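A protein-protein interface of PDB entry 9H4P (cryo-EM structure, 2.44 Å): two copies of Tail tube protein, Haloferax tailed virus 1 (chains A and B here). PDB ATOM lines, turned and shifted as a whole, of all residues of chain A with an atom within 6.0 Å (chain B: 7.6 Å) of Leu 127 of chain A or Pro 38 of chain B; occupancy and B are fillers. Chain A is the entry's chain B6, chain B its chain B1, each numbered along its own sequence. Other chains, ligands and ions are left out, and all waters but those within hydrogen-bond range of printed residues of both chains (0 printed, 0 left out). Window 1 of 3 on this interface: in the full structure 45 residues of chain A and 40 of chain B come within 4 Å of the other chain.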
ATOM      1  N   TYR A  69       8.785 -29.687  -0.388  1.00  0.00           N
ATOM      2  CA  TYR A  69      10.119 -29.292  -0.824  1.00  0.00           C
ATOM      3  C   TYR A  69      11.167 -29.733   0.202  1.00  0.00           C
ATOM      4  O   TYR A  69      10.841 -29.936   1.375  1.00  0.00           O
ATOM      5  CB  TYR A  69      10.149 -27.787  -1.135  1.00  0.00           C
ATOM      6  CG  TYR A  69      10.074 -26.878   0.069  1.00  0.00           C
ATOM      7  CD1 TYR A  69       8.881 -26.681   0.760  1.00  0.00           C
ATOM      8  CD2 TYR A  69      11.205 -26.204   0.516  1.00  0.00           C
ATOM      9  CE1 TYR A  69       8.818 -25.842   1.865  1.00  0.00           C
ATOM     10  CE2 TYR A  69      11.159 -25.366   1.622  1.00  0.00           C
ATOM     11  CZ  TYR A  69       9.962 -25.186   2.300  1.00  0.00           C
ATOM     12  OH  TYR A  69       9.912 -24.357   3.386  1.00  0.00           O
ATOM     13  N   PHE A  76      12.970 -17.326   2.478  1.00  0.00           N
ATOM     14  CA  PHE A  76      11.540 -17.608   2.454  1.00  0.00           C
ATOM     15  C   PHE A  76      10.949 -17.650   3.870  1.00  0.00           C
ATOM     16  O   PHE A  76       9.850 -17.133   4.092  1.00  0.00           O
ATOM     17  CB  PHE A  76      11.255 -18.894   1.671  1.00  0.00           C
ATOM     18  CG  PHE A  76       9.797 -19.283   1.654  1.00  0.00           C
ATOM     19  CD1 PHE A  76       8.944 -18.788   0.673  1.00  0.00           C
ATOM     20  CD2 PHE A  76       9.271 -20.125   2.632  1.00  0.00           C
ATOM     21  CE1 PHE A  76       7.599 -19.137   0.661  1.00  0.00           C
ATOM     22  CE2 PHE A  76       7.924 -20.468   2.624  1.00  0.00           C
ATOM     23  CZ  PHE A  76       7.091 -19.975   1.636  1.00  0.00           C
ATOM     24  N   ALA A  77      11.682 -18.277   4.806  1.00  0.00           N
ATOM     25  CA  ALA A  77      11.270 -18.394   6.198  1.00  0.00           C
ATOM     26  C   ALA A  77      11.244 -17.033   6.905  1.00  0.00           C
ATOM     27  O   ALA A  77      10.274 -16.740   7.608  1.00  0.00           O
ATOM     28  CB  ALA A  77      12.141 -19.405   6.914  1.00  0.00           C
ATOM     29  N   GLN A  78      12.293 -16.210   6.713  1.00  0.00           N
ATOM     30  CA  GLN A  78      12.399 -14.907   7.368  1.00  0.00           C
ATOM     31  C   GLN A  78      11.436 -13.880   6.759  1.00  0.00           C
ATOM     32  O   GLN A  78      11.020 -12.949   7.453  1.00  0.00           O
ATOM     33  CB  GLN A  78      13.852 -14.425   7.407  1.00  0.00           C
ATOM     34  CG  GLN A  78      14.747 -15.271   8.304  1.00  0.00           C
ATOM     35  CD  GLN A  78      16.205 -14.882   8.227  1.00  0.00           C
ATOM     36  OE1 GLN A  78      16.636 -14.143   7.342  1.00  0.00           O
ATOM     37  NE2 GLN A  78      16.989 -15.385   9.166  1.00  0.00           N
ATOM     38  N   TRP A  80       8.399 -14.964   5.624  1.00  0.00           N
ATOM     39  CA  TRP A  80       7.157 -15.430   6.231  1.00  0.00           C
ATOM     40  C   TRP A  80       6.996 -14.890   7.656  1.00  0.00           C
ATOM     41  O   TRP A  80       5.898 -14.460   8.022  1.00  0.00           O
ATOM     42  CB  TRP A  80       7.052 -16.965   6.186  1.00  0.00           C
ATOM     43  CG  TRP A  80       5.767 -17.501   6.752  1.00  0.00           C
ATOM     44  CD1 TRP A  80       4.630 -17.780   6.047  1.00  0.00           C
ATOM     45  CD2 TRP A  80       5.465 -17.823   8.134  1.00  0.00           C
ATOM     46  NE1 TRP A  80       3.649 -18.248   6.883  1.00  0.00           N
ATOM     47  CE2 TRP A  80       4.127 -18.290   8.171  1.00  0.00           C
ATOM     48  CE3 TRP A  80       6.177 -17.769   9.347  1.00  0.00           C
ATOM     49  CZ2 TRP A  80       3.501 -18.693   9.360  1.00  0.00           C
ATOM     50  CZ3 TRP A  80       5.561 -18.169  10.521  1.00  0.00           C
ATOM     51  CH2 TRP A  80       4.237 -18.626  10.526  1.00  0.00           C
ATOM     52  N   LEU A  81       8.083 -14.928   8.451  1.00  0.00           N
ATOM     53  CA  LEU A  81       8.074 -14.400   9.812  1.00  0.00           C
ATOM     54  C   LEU A  81       7.792 -12.893   9.819  1.00  0.00           C
ATOM     55  O   LEU A  81       7.025 -12.417  10.659  1.00  0.00           O
ATOM     56  CB  LEU A  81       9.405 -14.711  10.513  1.00  0.00           C
ATOM     57  CG  LEU A  81       9.622 -16.158  10.968  1.00  0.00           C
ATOM     58  CD1 LEU A  81      11.084 -16.382  11.335  1.00  0.00           C
ATOM     59  CD2 LEU A  81       8.725 -16.517  12.151  1.00  0.00           C
ATOM     60  N   SER A  91       9.199 -14.549  15.513  1.00  0.00           N
ATOM     61  CA  SER A  91       7.768 -14.370  15.280  1.00  0.00           C
ATOM     62  C   SER A  91       7.367 -12.924  15.571  1.00  0.00           C
ATOM     63  O   SER A  91       7.808 -12.340  16.562  1.00  0.00           O
ATOM     64  CB  SER A  91       6.920 -15.310  16.113  1.00  0.00           C
ATOM     65  OG  SER A  91       7.178 -16.672  15.794  1.00  0.00           O
ATOM     66  N   PHE A 124       0.420 -18.627   3.693  1.00  0.00           N
ATOM     67  CA  PHE A 124       0.575 -19.928   4.332  1.00  0.00           C
ATOM     68  C   PHE A 124       0.263 -19.789   5.826  1.00  0.00           C
ATOM     69  O   PHE A 124       0.930 -19.006   6.507  1.00  0.00           O
ATOM     70  CB  PHE A 124       1.984 -20.472   4.060  1.00  0.00           C
ATOM     71  CG  PHE A 124       2.328 -20.573   2.593  1.00  0.00           C
ATOM     72  CD1 PHE A 124       1.833 -21.624   1.827  1.00  0.00           C
ATOM     73  CD2 PHE A 124       3.122 -19.612   1.965  1.00  0.00           C
ATOM     74  CE1 PHE A 124       2.129 -21.723   0.472  1.00  0.00           C
ATOM     75  CE2 PHE A 124       3.418 -19.712   0.610  1.00  0.00           C
ATOM     76  CZ  PHE A 124       2.929 -20.771  -0.133  1.00  0.00           C
ATOM     77  N   PRO A 125      -0.784 -20.473   6.377  1.00  0.00           N
ATOM     78  CA  PRO A 125      -1.089 -20.405   7.816  1.00  0.00           C
ATOM     79  C   PRO A 125       0.045 -20.857   8.739  1.00  0.00           C
ATOM     80  O   PRO A 125       0.196 -20.318   9.840  1.00  0.00           O
ATOM     81  CB  PRO A 125      -2.343 -21.290   7.989  1.00  0.00           C
ATOM     82  CG  PRO A 125      -2.975 -21.309   6.605  1.00  0.00           C
ATOM     83  CD  PRO A 125      -1.796 -21.266   5.648  1.00  0.00           C
ATOM     84  N   GLU A 126       0.840 -21.832   8.271  1.00  0.00           N
ATOM     85  CA  GLU A 126       1.919 -22.397   9.068  1.00  0.00           C
ATOM     86  C   GLU A 126       3.139 -22.684   8.193  1.00  0.00           C
ATOM     87  O   GLU A 126       3.017 -23.078   7.028  1.00  0.00           O
ATOM     88  CB  GLU A 126       1.440 -23.623   9.855  1.00  0.00           C
ATOM     89  CG  GLU A 126       1.039 -24.825   9.006  1.00  0.00           C
ATOM     90  CD  GLU A 126       0.432 -25.974   9.789  1.00  0.00           C
ATOM     91  OE1 GLU A 126      -0.374 -25.714  10.702  1.00  0.00           O
ATOM     92  OE2 GLU A 126       0.769 -27.125   9.481  1.00  0.00           O
ATOM     93  N   LEU A 127       4.314 -22.477   8.797  1.00  0.00           N
ATOM     94  CA  LEU A 127       5.599 -22.675   8.146  1.00  0.00           C
ATOM     95  C   LEU A 127       6.368 -23.738   8.931  1.00  0.00           C
ATOM     96  O   LEU A 127       6.691 -23.515  10.102  1.00  0.00           O
ATOM     97  CB  LEU A 127       6.343 -21.328   8.141  1.00  0.00           C
ATOM     98  CG  LEU A 127       7.812 -21.351   7.698  1.00  0.00           C
ATOM     99  CD1 LEU A 127       7.945 -21.487   6.182  1.00  0.00           C
ATOM    100  CD2 LEU A 127       8.540 -20.099   8.172  1.00  0.00           C
ATOM    101  N   PRO A 128       6.675 -24.927   8.345  1.00  0.00           N
ATOM    102  CA  PRO A 128       7.547 -25.887   9.024  1.00  0.00           C
ATOM    103  C   PRO A 128       8.986 -25.369   8.978  1.00  0.00           C
ATOM    104  O   PRO A 128       9.548 -25.164   7.898  1.00  0.00           O
ATOM    105  CB  PRO A 128       7.352 -27.190   8.223  1.00  0.00           C
ATOM    106  CG  PRO A 128       6.957 -26.730   6.826  1.00  0.00           C
ATOM    107  CD  PRO A 128       6.216 -25.419   7.029  1.00  0.00           C
ATOM    108  N   LEU A 129       9.564 -25.128  10.163  1.00  0.00           N
ATOM    109  CA  LEU A 129      10.942 -24.662  10.251  1.00  0.00           C
ATOM    110  C   LEU A 129      11.894 -25.853  10.285  1.00  0.00           C
ATOM    111  O   LEU A 129      12.833 -25.914   9.491  1.00  0.00           O
ATOM    112  CB  LEU A 129      11.122 -23.753  11.475  1.00  0.00           C
ATOM    113  CG  LEU A 129      10.526 -22.349  11.348  1.00  0.00           C
ATOM    114  CD1 LEU A 129      10.810 -21.520  12.595  1.00  0.00           C
ATOM    115  CD2 LEU A 129      11.048 -21.627  10.111  1.00  0.00           C
ATOM    116  N   LEU A 142       4.082 -27.178   2.727  1.00  0.00           N
ATOM    117  CA  LEU A 142       3.279 -25.966   2.850  1.00  0.00           C
ATOM    118  C   LEU A 142       1.871 -26.259   2.332  1.00  0.00           C
ATOM    119  O   LEU A 142       1.720 -26.950   1.324  1.00  0.00           O
ATOM    120  CB  LEU A 142       3.909 -24.847   2.003  1.00  0.00           C
ATOM    121  CG  LEU A 142       5.244 -24.269   2.484  1.00  0.00           C
ATOM    122  CD1 LEU A 142       5.976 -23.558   1.348  1.00  0.00           C
ATOM    123  CD2 LEU A 142       5.055 -23.321   3.669  1.00  0.00           C
ATOM    124  N   THR B  35       9.754 -32.057  14.777  1.00  0.00           N
ATOM    125  CA  THR B  35       9.013 -31.106  13.957  1.00  0.00           C
ATOM    126  C   THR B  35       8.770 -29.830  14.767  1.00  0.00           C
ATOM    127  O   THR B  35       8.225 -29.894  15.873  1.00  0.00           O
ATOM    128  CB  THR B  35       7.686 -31.700  13.456  1.00  0.00           C
ATOM    129  OG1 THR B  35       7.955 -32.821  12.612  1.00  0.00           O
ATOM    130  CG2 THR B  35       6.813 -30.707  12.714  1.00  0.00           C
ATOM    131  N   ILE B  36       9.179 -28.679  14.208  1.00  0.00           N
ATOM    132  CA  ILE B  36       8.870 -27.367  14.767  1.00  0.00           C
ATOM    133  C   ILE B  36       8.141 -26.558  13.691  1.00  0.00           C
ATOM    134  O   ILE B  36       8.672 -26.363  12.593  1.00  0.00           O
ATOM    135  CB  ILE B  36      10.141 -26.642  15.286  1.00  0.00           C
ATOM    136  CG1 ILE B  36      10.919 -27.470  16.323  1.00  0.00           C
ATOM    137  CG2 ILE B  36       9.802 -25.243  15.811  1.00  0.00           C
ATOM    138  CD1 ILE B  36      12.372 -27.053  16.528  1.00  0.00           C
ATOM    139  N   THR B  37       6.925 -26.094  14.013  1.00  0.00           N
ATOM    140  CA  THR B  37       6.078 -25.407  13.047  1.00  0.00           C
ATOM    141  C   THR B  37       5.416 -24.194  13.707  1.00  0.00           C
ATOM    142  O   THR B  37       4.430 -24.353  14.435  1.00  0.00           O
ATOM    143  CB  THR B  37       5.018 -26.357  12.462  1.00  0.00           C
ATOM    144  OG1 THR B  37       5.671 -27.461  11.834  1.00  0.00           O
ATOM    145  CG2 THR B  37       4.087 -25.697  11.466  1.00  0.00           C
ATOM    146  N   PRO B  38       5.932 -22.952  13.502  1.00  0.00           N
ATOM    147  CA  PRO B  38       5.149 -21.748  13.795  1.00  0.00           C
ATOM    148  C   PRO B  38       3.908 -21.695  12.902  1.00  0.00           C
ATOM    149  O   PRO B  38       3.966 -21.997  11.705  1.00  0.00           O
ATOM    150  CB  PRO B  38       6.106 -20.572  13.511  1.00  0.00           C
ATOM    151  CG  PRO B  38       7.162 -21.167  12.591  1.00  0.00           C
ATOM    152  CD  PRO B  38       7.290 -22.617  13.033  1.00  0.00           C
ATOM    153  N   ALA B  39       2.792 -21.314  13.534  1.00  0.00           N
ATOM    154  CA  ALA B  39       1.481 -21.313  12.909  1.00  0.00           C
ATOM    155  C   ALA B  39       0.675 -20.117  13.409  1.00  0.00           C
ATOM    156  O   ALA B  39       0.833 -19.674  14.550  1.00  0.00           O
ATOM    157  CB  ALA B  39       0.767 -22.615  13.213  1.00  0.00           C
ATOM    158  N   TYR B  40      -0.201 -19.626  12.528  1.00  0.00           N
ATOM    159  CA  TYR B  40      -1.280 -18.729  12.898  1.00  0.00           C
ATOM    160  C   TYR B  40      -2.561 -19.280  12.276  1.00  0.00           C
ATOM    161  O   TYR B  40      -2.512 -19.955  11.241  1.00  0.00           O
ATOM    162  CB  TYR B  40      -1.035 -17.326  12.329  1.00  0.00           C
ATOM    163  CG  TYR B  40       0.211 -16.576  12.744  1.00  0.00           C
ATOM    164  CD1 TYR B  40       1.445 -16.817  12.140  1.00  0.00           C
ATOM    165  CD2 TYR B  40       0.128 -15.537  13.668  1.00  0.00           C
ATOM    166  CE1 TYR B  40       2.568 -16.074  12.475  1.00  0.00           C
ATOM    167  CE2 TYR B  40       1.241 -14.780  14.012  1.00  0.00           C
ATOM    168  CZ  TYR B  40       2.463 -15.055  13.414  1.00  0.00           C
ATOM    169  OH  TYR B  40       3.573 -14.338  13.757  1.00  0.00           O
ATOM    170  N   HIS B  61      -1.511 -17.038  17.457  1.00  0.00           N
ATOM    171  CA  HIS B  61      -0.201 -17.584  17.120  1.00  0.00           C
ATOM    172  C   HIS B  61       0.150 -18.765  18.030  1.00  0.00           C
ATOM    173  O   HIS B  61      -0.208 -18.781  19.210  1.00  0.00           O
ATOM    174  CB  HIS B  61       0.880 -16.490  17.169  1.00  0.00           C
ATOM    175  CG  HIS B  61       2.220 -16.955  16.694  1.00  0.00           C
ATOM    176  ND1 HIS B  61       2.447 -17.381  15.392  1.00  0.00           N
ATOM    177  CD2 HIS B  61       3.399 -17.078  17.344  1.00  0.00           C
ATOM    178  CE1 HIS B  61       3.714 -17.727  15.257  1.00  0.00           C
ATOM    179  NE2 HIS B  61       4.318 -17.555  16.445  1.00  0.00           N
ATOM    180  N   ASN B  62       0.893 -19.720  17.453  1.00  0.00           N
ATOM    181  CA  ASN B  62       1.240 -20.989  18.072  1.00  0.00           C
ATOM    182  C   ASN B  62       2.553 -21.465  17.446  1.00  0.00           C
ATOM    183  O   ASN B  62       2.856 -21.103  16.308  1.00  0.00           O
ATOM    184  CB  ASN B  62       0.099 -21.990  17.836  1.00  0.00           C
ATOM    185  CG  ASN B  62       0.323 -23.375  18.410  1.00  0.00           C
ATOM    186  OD1 ASN B  62       1.118 -23.570  19.329  1.00  0.00           O
ATOM    187  ND2 ASN B  62      -0.386 -24.357  17.875  1.00  0.00           N
ATOM    188  N   VAL B  63       3.334 -22.266  18.189  1.00  0.00           N
ATOM    189  CA  VAL B  63       4.445 -23.009  17.602  1.00  0.00           C
ATOM    190  C   VAL B  63       4.263 -24.480  17.979  1.00  0.00           C
ATOM    191  O   VAL B  63       4.566 -24.868  19.110  1.00  0.00           O
ATOM    192  CB  VAL B  63       5.840 -22.479  18.023  1.00  0.00           C
ATOM    193  CG1 VAL B  63       6.985 -23.253  17.366  1.00  0.00           C
ATOM    194  CG2 VAL B  63       6.010 -20.980  17.782  1.00  0.00           C
ATOM    195  N   ASN B  64       3.755 -25.282  17.032  1.00  0.00           N
ATOM    196  CA  ASN B  64       3.642 -26.719  17.242  1.00  0.00           C
ATOM    197  C   ASN B  64       5.043 -27.326  17.319  1.00  0.00           C
ATOM    198  O   ASN B  64       5.834 -27.196  16.382  1.00  0.00           O
ATOM    199  CB  ASN B  64       2.824 -27.397  16.137  1.00  0.00           C
ATOM    200  CG  ASN B  64       1.377 -26.946  16.096  1.00  0.00           C
ATOM    201  OD1 ASN B  64       1.019 -26.067  15.314  1.00  0.00           O
ATOM    202  ND2 ASN B  64       0.538 -27.536  16.931  1.00  0.00           N
ATOM    203  N   VAL B  65       5.334 -27.971  18.456  1.00  0.00           N
ATOM    204  CA  VAL B  65       6.558 -28.736  18.648  1.00  0.00           C
ATOM    205  C   VAL B  65       6.147 -30.193  18.853  1.00  0.00           C
ATOM    206  O   VAL B  65       5.335 -30.487  19.735  1.00  0.00           O
ATOM    207  CB  VAL B  65       7.371 -28.207  19.854  1.00  0.00           C
ATOM    208  CG1 VAL B  65       8.563 -29.100  20.200  1.00  0.00           C
ATOM    209  CG2 VAL B  65       7.819 -26.755  19.680  1.00  0.00           C
ATOM    210  N   THR B 117      17.124 -22.707  15.168  1.00  0.00           N
ATOM    211  CA  THR B 117      15.748 -22.392  15.539  1.00  0.00           C
ATOM    212  C   THR B 117      15.627 -22.406  17.066  1.00  0.00           C
ATOM    213  O   THR B 117      16.017 -23.386  17.701  1.00  0.00           O
ATOM    214  CB  THR B 117      14.762 -23.419  14.956  1.00  0.00           C
ATOM    215  OG1 THR B 117      14.913 -23.490  13.536  1.00  0.00           O
ATOM    216  CG2 THR B 117      13.311 -23.126  15.283  1.00  0.00           C
ATOM    217  N   VAL B 119      12.726 -21.613  20.327  1.00  0.00           N
ATOM    218  CA  VAL B 119      11.305 -21.502  20.650  1.00  0.00           C
ATOM    219  C   VAL B 119      11.165 -21.271  22.159  1.00  0.00           C
ATOM    220  O   VAL B 119      11.785 -21.983  22.952  1.00  0.00           O
ATOM    221  CB  VAL B 119      10.514 -22.755  20.198  1.00  0.00           C
ATOM    222  CG1 VAL B 119       9.018 -22.639  20.489  1.00  0.00           C
ATOM    223  CG2 VAL B 119      10.732 -23.100  18.725  1.00  0.00           C
ATOM    224  N   GLY B 146       4.774 -24.062  21.776  1.00  0.00           N
ATOM    225  CA  GLY B 146       5.551 -22.894  22.176  1.00  0.00           C
ATOM    226  C   GLY B 146       4.780 -21.593  21.947  1.00  0.00           C
ATOM    227  O   GLY B 146       3.793 -21.572  21.206  1.00  0.00           O
ATOM    228  N   SER B 148       6.351 -18.493  20.880  1.00  0.00           N
ATOM    229  CA  SER B 148       6.904 -17.821  19.706  1.00  0.00           C
ATOM    230  C   SER B 148       8.258 -18.423  19.318  1.00  0.00           C
ATOM    231  O   SER B 148       8.904 -19.086  20.132  1.00  0.00           O
ATOM    232  CB  SER B 148       6.994 -16.309  19.913  1.00  0.00           C
ATOM    233  OG  SER B 148       8.074 -15.959  20.769  1.00  0.00           O
ATOM    234  N   VAL B 149       8.667 -18.188  18.059  1.00  0.00           N
ATOM    235  CA  VAL B 149      10.037 -18.413  17.611  1.00  0.00           C
ATOM    236  C   VAL B 149      10.848 -17.176  18.007  1.00  0.00           C
ATOM    237  O   VAL B 149      10.561 -16.077  17.527  1.00  0.00           O
ATOM    238  CB  VAL B 149      10.115 -18.683  16.088  1.00  0.00           C
ATOM    239  CG1 VAL B 149      11.554 -18.781  15.584  1.00  0.00           C
ATOM    240  CG2 VAL B 149       9.326 -19.925  15.680  1.00  0.00           C
ATOM    241  N   LEU B 152      15.455 -17.432  14.444  1.00  0.00           N
ATOM    242  CA  LEU B 152      15.678 -18.243  13.256  1.00  0.00           C
ATOM    243  C   LEU B 152      16.710 -17.522  12.387  1.00  0.00           C
ATOM    244  O   LEU B 152      16.391 -16.524  11.733  1.00  0.00           O
ATOM    245  CB  LEU B 152      14.365 -18.468  12.493  1.00  0.00           C
ATOM    246  CG  LEU B 152      14.540 -19.203  11.159  1.00  0.00           C
ATOM    247  CD1 LEU B 152      14.813 -20.693  11.359  1.00  0.00           C
ATOM    248  CD2 LEU B 152      13.354 -18.979  10.233  1.00  0.00           C
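No position is printed for both chains.
Of the 21 pairs that touch across the chains among the printed residues, none has its exchanged pair printed and touching as well.
The indole nitrogen (NE1) of Trp 80 of chain A lies within hydrogen-bond range of the backbone carbonyl oxygen (O) of Phe 124 of chain A (2.8 Å).
N of Ala 39 of chain B is in hydrogen-bond range of O of Asn 62 of chain B (2.8 Å).
ND1 of His 61 of chain B is in hydrogen-bond range of O of Ala 39 of chain B, at 2.9 Å.
N of Thr 37 of chain B sits at hydrogen-bond distance from O of Asn 64 of chain B (2.8 Å).
The backbone NH of Tyr 40 of chain B lies within hydrogen-bond range of the backbone carbonyl oxygen of Pro 125 of chain A, 2.8 Å away.
The backbone carbonyl oxygen (O) of Leu 152 of chain B is in hydrogen-bond range of the side-chain amide nitrogen (NE2) of Gln 78 of chain A.
N of Leu 127 of chain A is in hydrogen-bond range of O of Pro 38 of chain B, at 3.0 Å.
The backbone NH (N) of Leu 129 of chain A is in hydrogen-bond range of the backbone carbonyl oxygen (O) of Ile 36 of chain B (2.9 Å).
The backbone carbonyl oxygen (O) of Val 149 of chain B lies within hydrogen-bond range of the backbone NH (N) of Ser 91 of chain A.
NE2 of His 61 of chain B is in hydrogen-bond range of OG of Ser 91 of chain A, 3.1 Å away.
Of chain B, only Thr 37 and Pro 38 come within 4 Å of Leu 127 of chain A.
Pro 38 of chain B touches just these residues of chain A: Trp 80 (3.6 Å), Glu 126 (3.4 Å), Leu 127 (3.0 Å) and Leu 129 (3.7 Å).
Of the printed residues of chain B, Pro 125 of chain A touches Ala 39 and Tyr 40.
Of the printed residues of chain B, Leu 129 of chain A touches Ile 36, Pro 38, Val 149 and Leu 152.
Of the printed residues of chain A, Thr 37 of chain B touches Glu 126 (3.7 Å), Leu 127 (3.6 Å) and Pro 128 (3.7 Å).
Printed residues of chain B within 4 Å of Ala 77 of chain A: Leu 152.
Of the printed residues of chain B, Trp 80 of chain A touches Pro 38 and Tyr 40.
Asn 64 of chain B touches none of the printed residues of chain A.
The nearest residue of chain A that does not touch Pro 38 of chain B is Pro 125 of chain A (4.5 Å).
The nearest printed residue of chain B that does not touch Trp 80 of chain A is Ala 39 of chain B (4.3 Å).
Ala 77 of chain A touches Leu 152 of chain B (CB to CD2, 3.6 Å).
Trp 80 of chain A touches Pro 38 of chain B.
Tyr 40 of chain B touches Trp 80 of chain A.
Leu 152 of chain B touches Leu 81 of chain A (CD2 to CD1, 3.6 Å).
Ser 91 of chain A touches Ser 148 of chain B.
Glu 126 of chain A touches Thr 37 of chain B (CB to CG2, 3.7 Å).
Pro 128 of chain A touches Ile 36 of chain B (C to O, 3.8 Å).
Leu 129 of chain A touches Pro 38 of chain B.
CG2 of Val 149 of chain B touches CD1 of Leu 129 of chain A, 3.8 Å away.
Leu 152 of chain B touches Leu 129 of chain A.
Of the 17 printed residues of chain B, 9 touch a printed residue of chain A.
Hydrophobic or aromatic side chains of chain B that line the printed part of chain A: Pro 38, Ala 39, Tyr 40, His 61, Val 149 and Leu 152.
Printed residues of chain A that touch a printed residue of chain B: Ala 77, Gln 78, Trp 80, Leu 81, Ser 91, Pro 125, Glu 126, Leu 127, Pro 128 and Leu 129.
Hydrophobic or aromatic side chains of chain A that line the printed part of chain B: Ala 77, Trp 80, Leu 81, Pro 125, Pro 128 and Leu 129.
Among the printed residues, no Asp or Glu carboxylate lies within 4 Å of a Lys or Arg side-chain nitrogen of the other chain.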
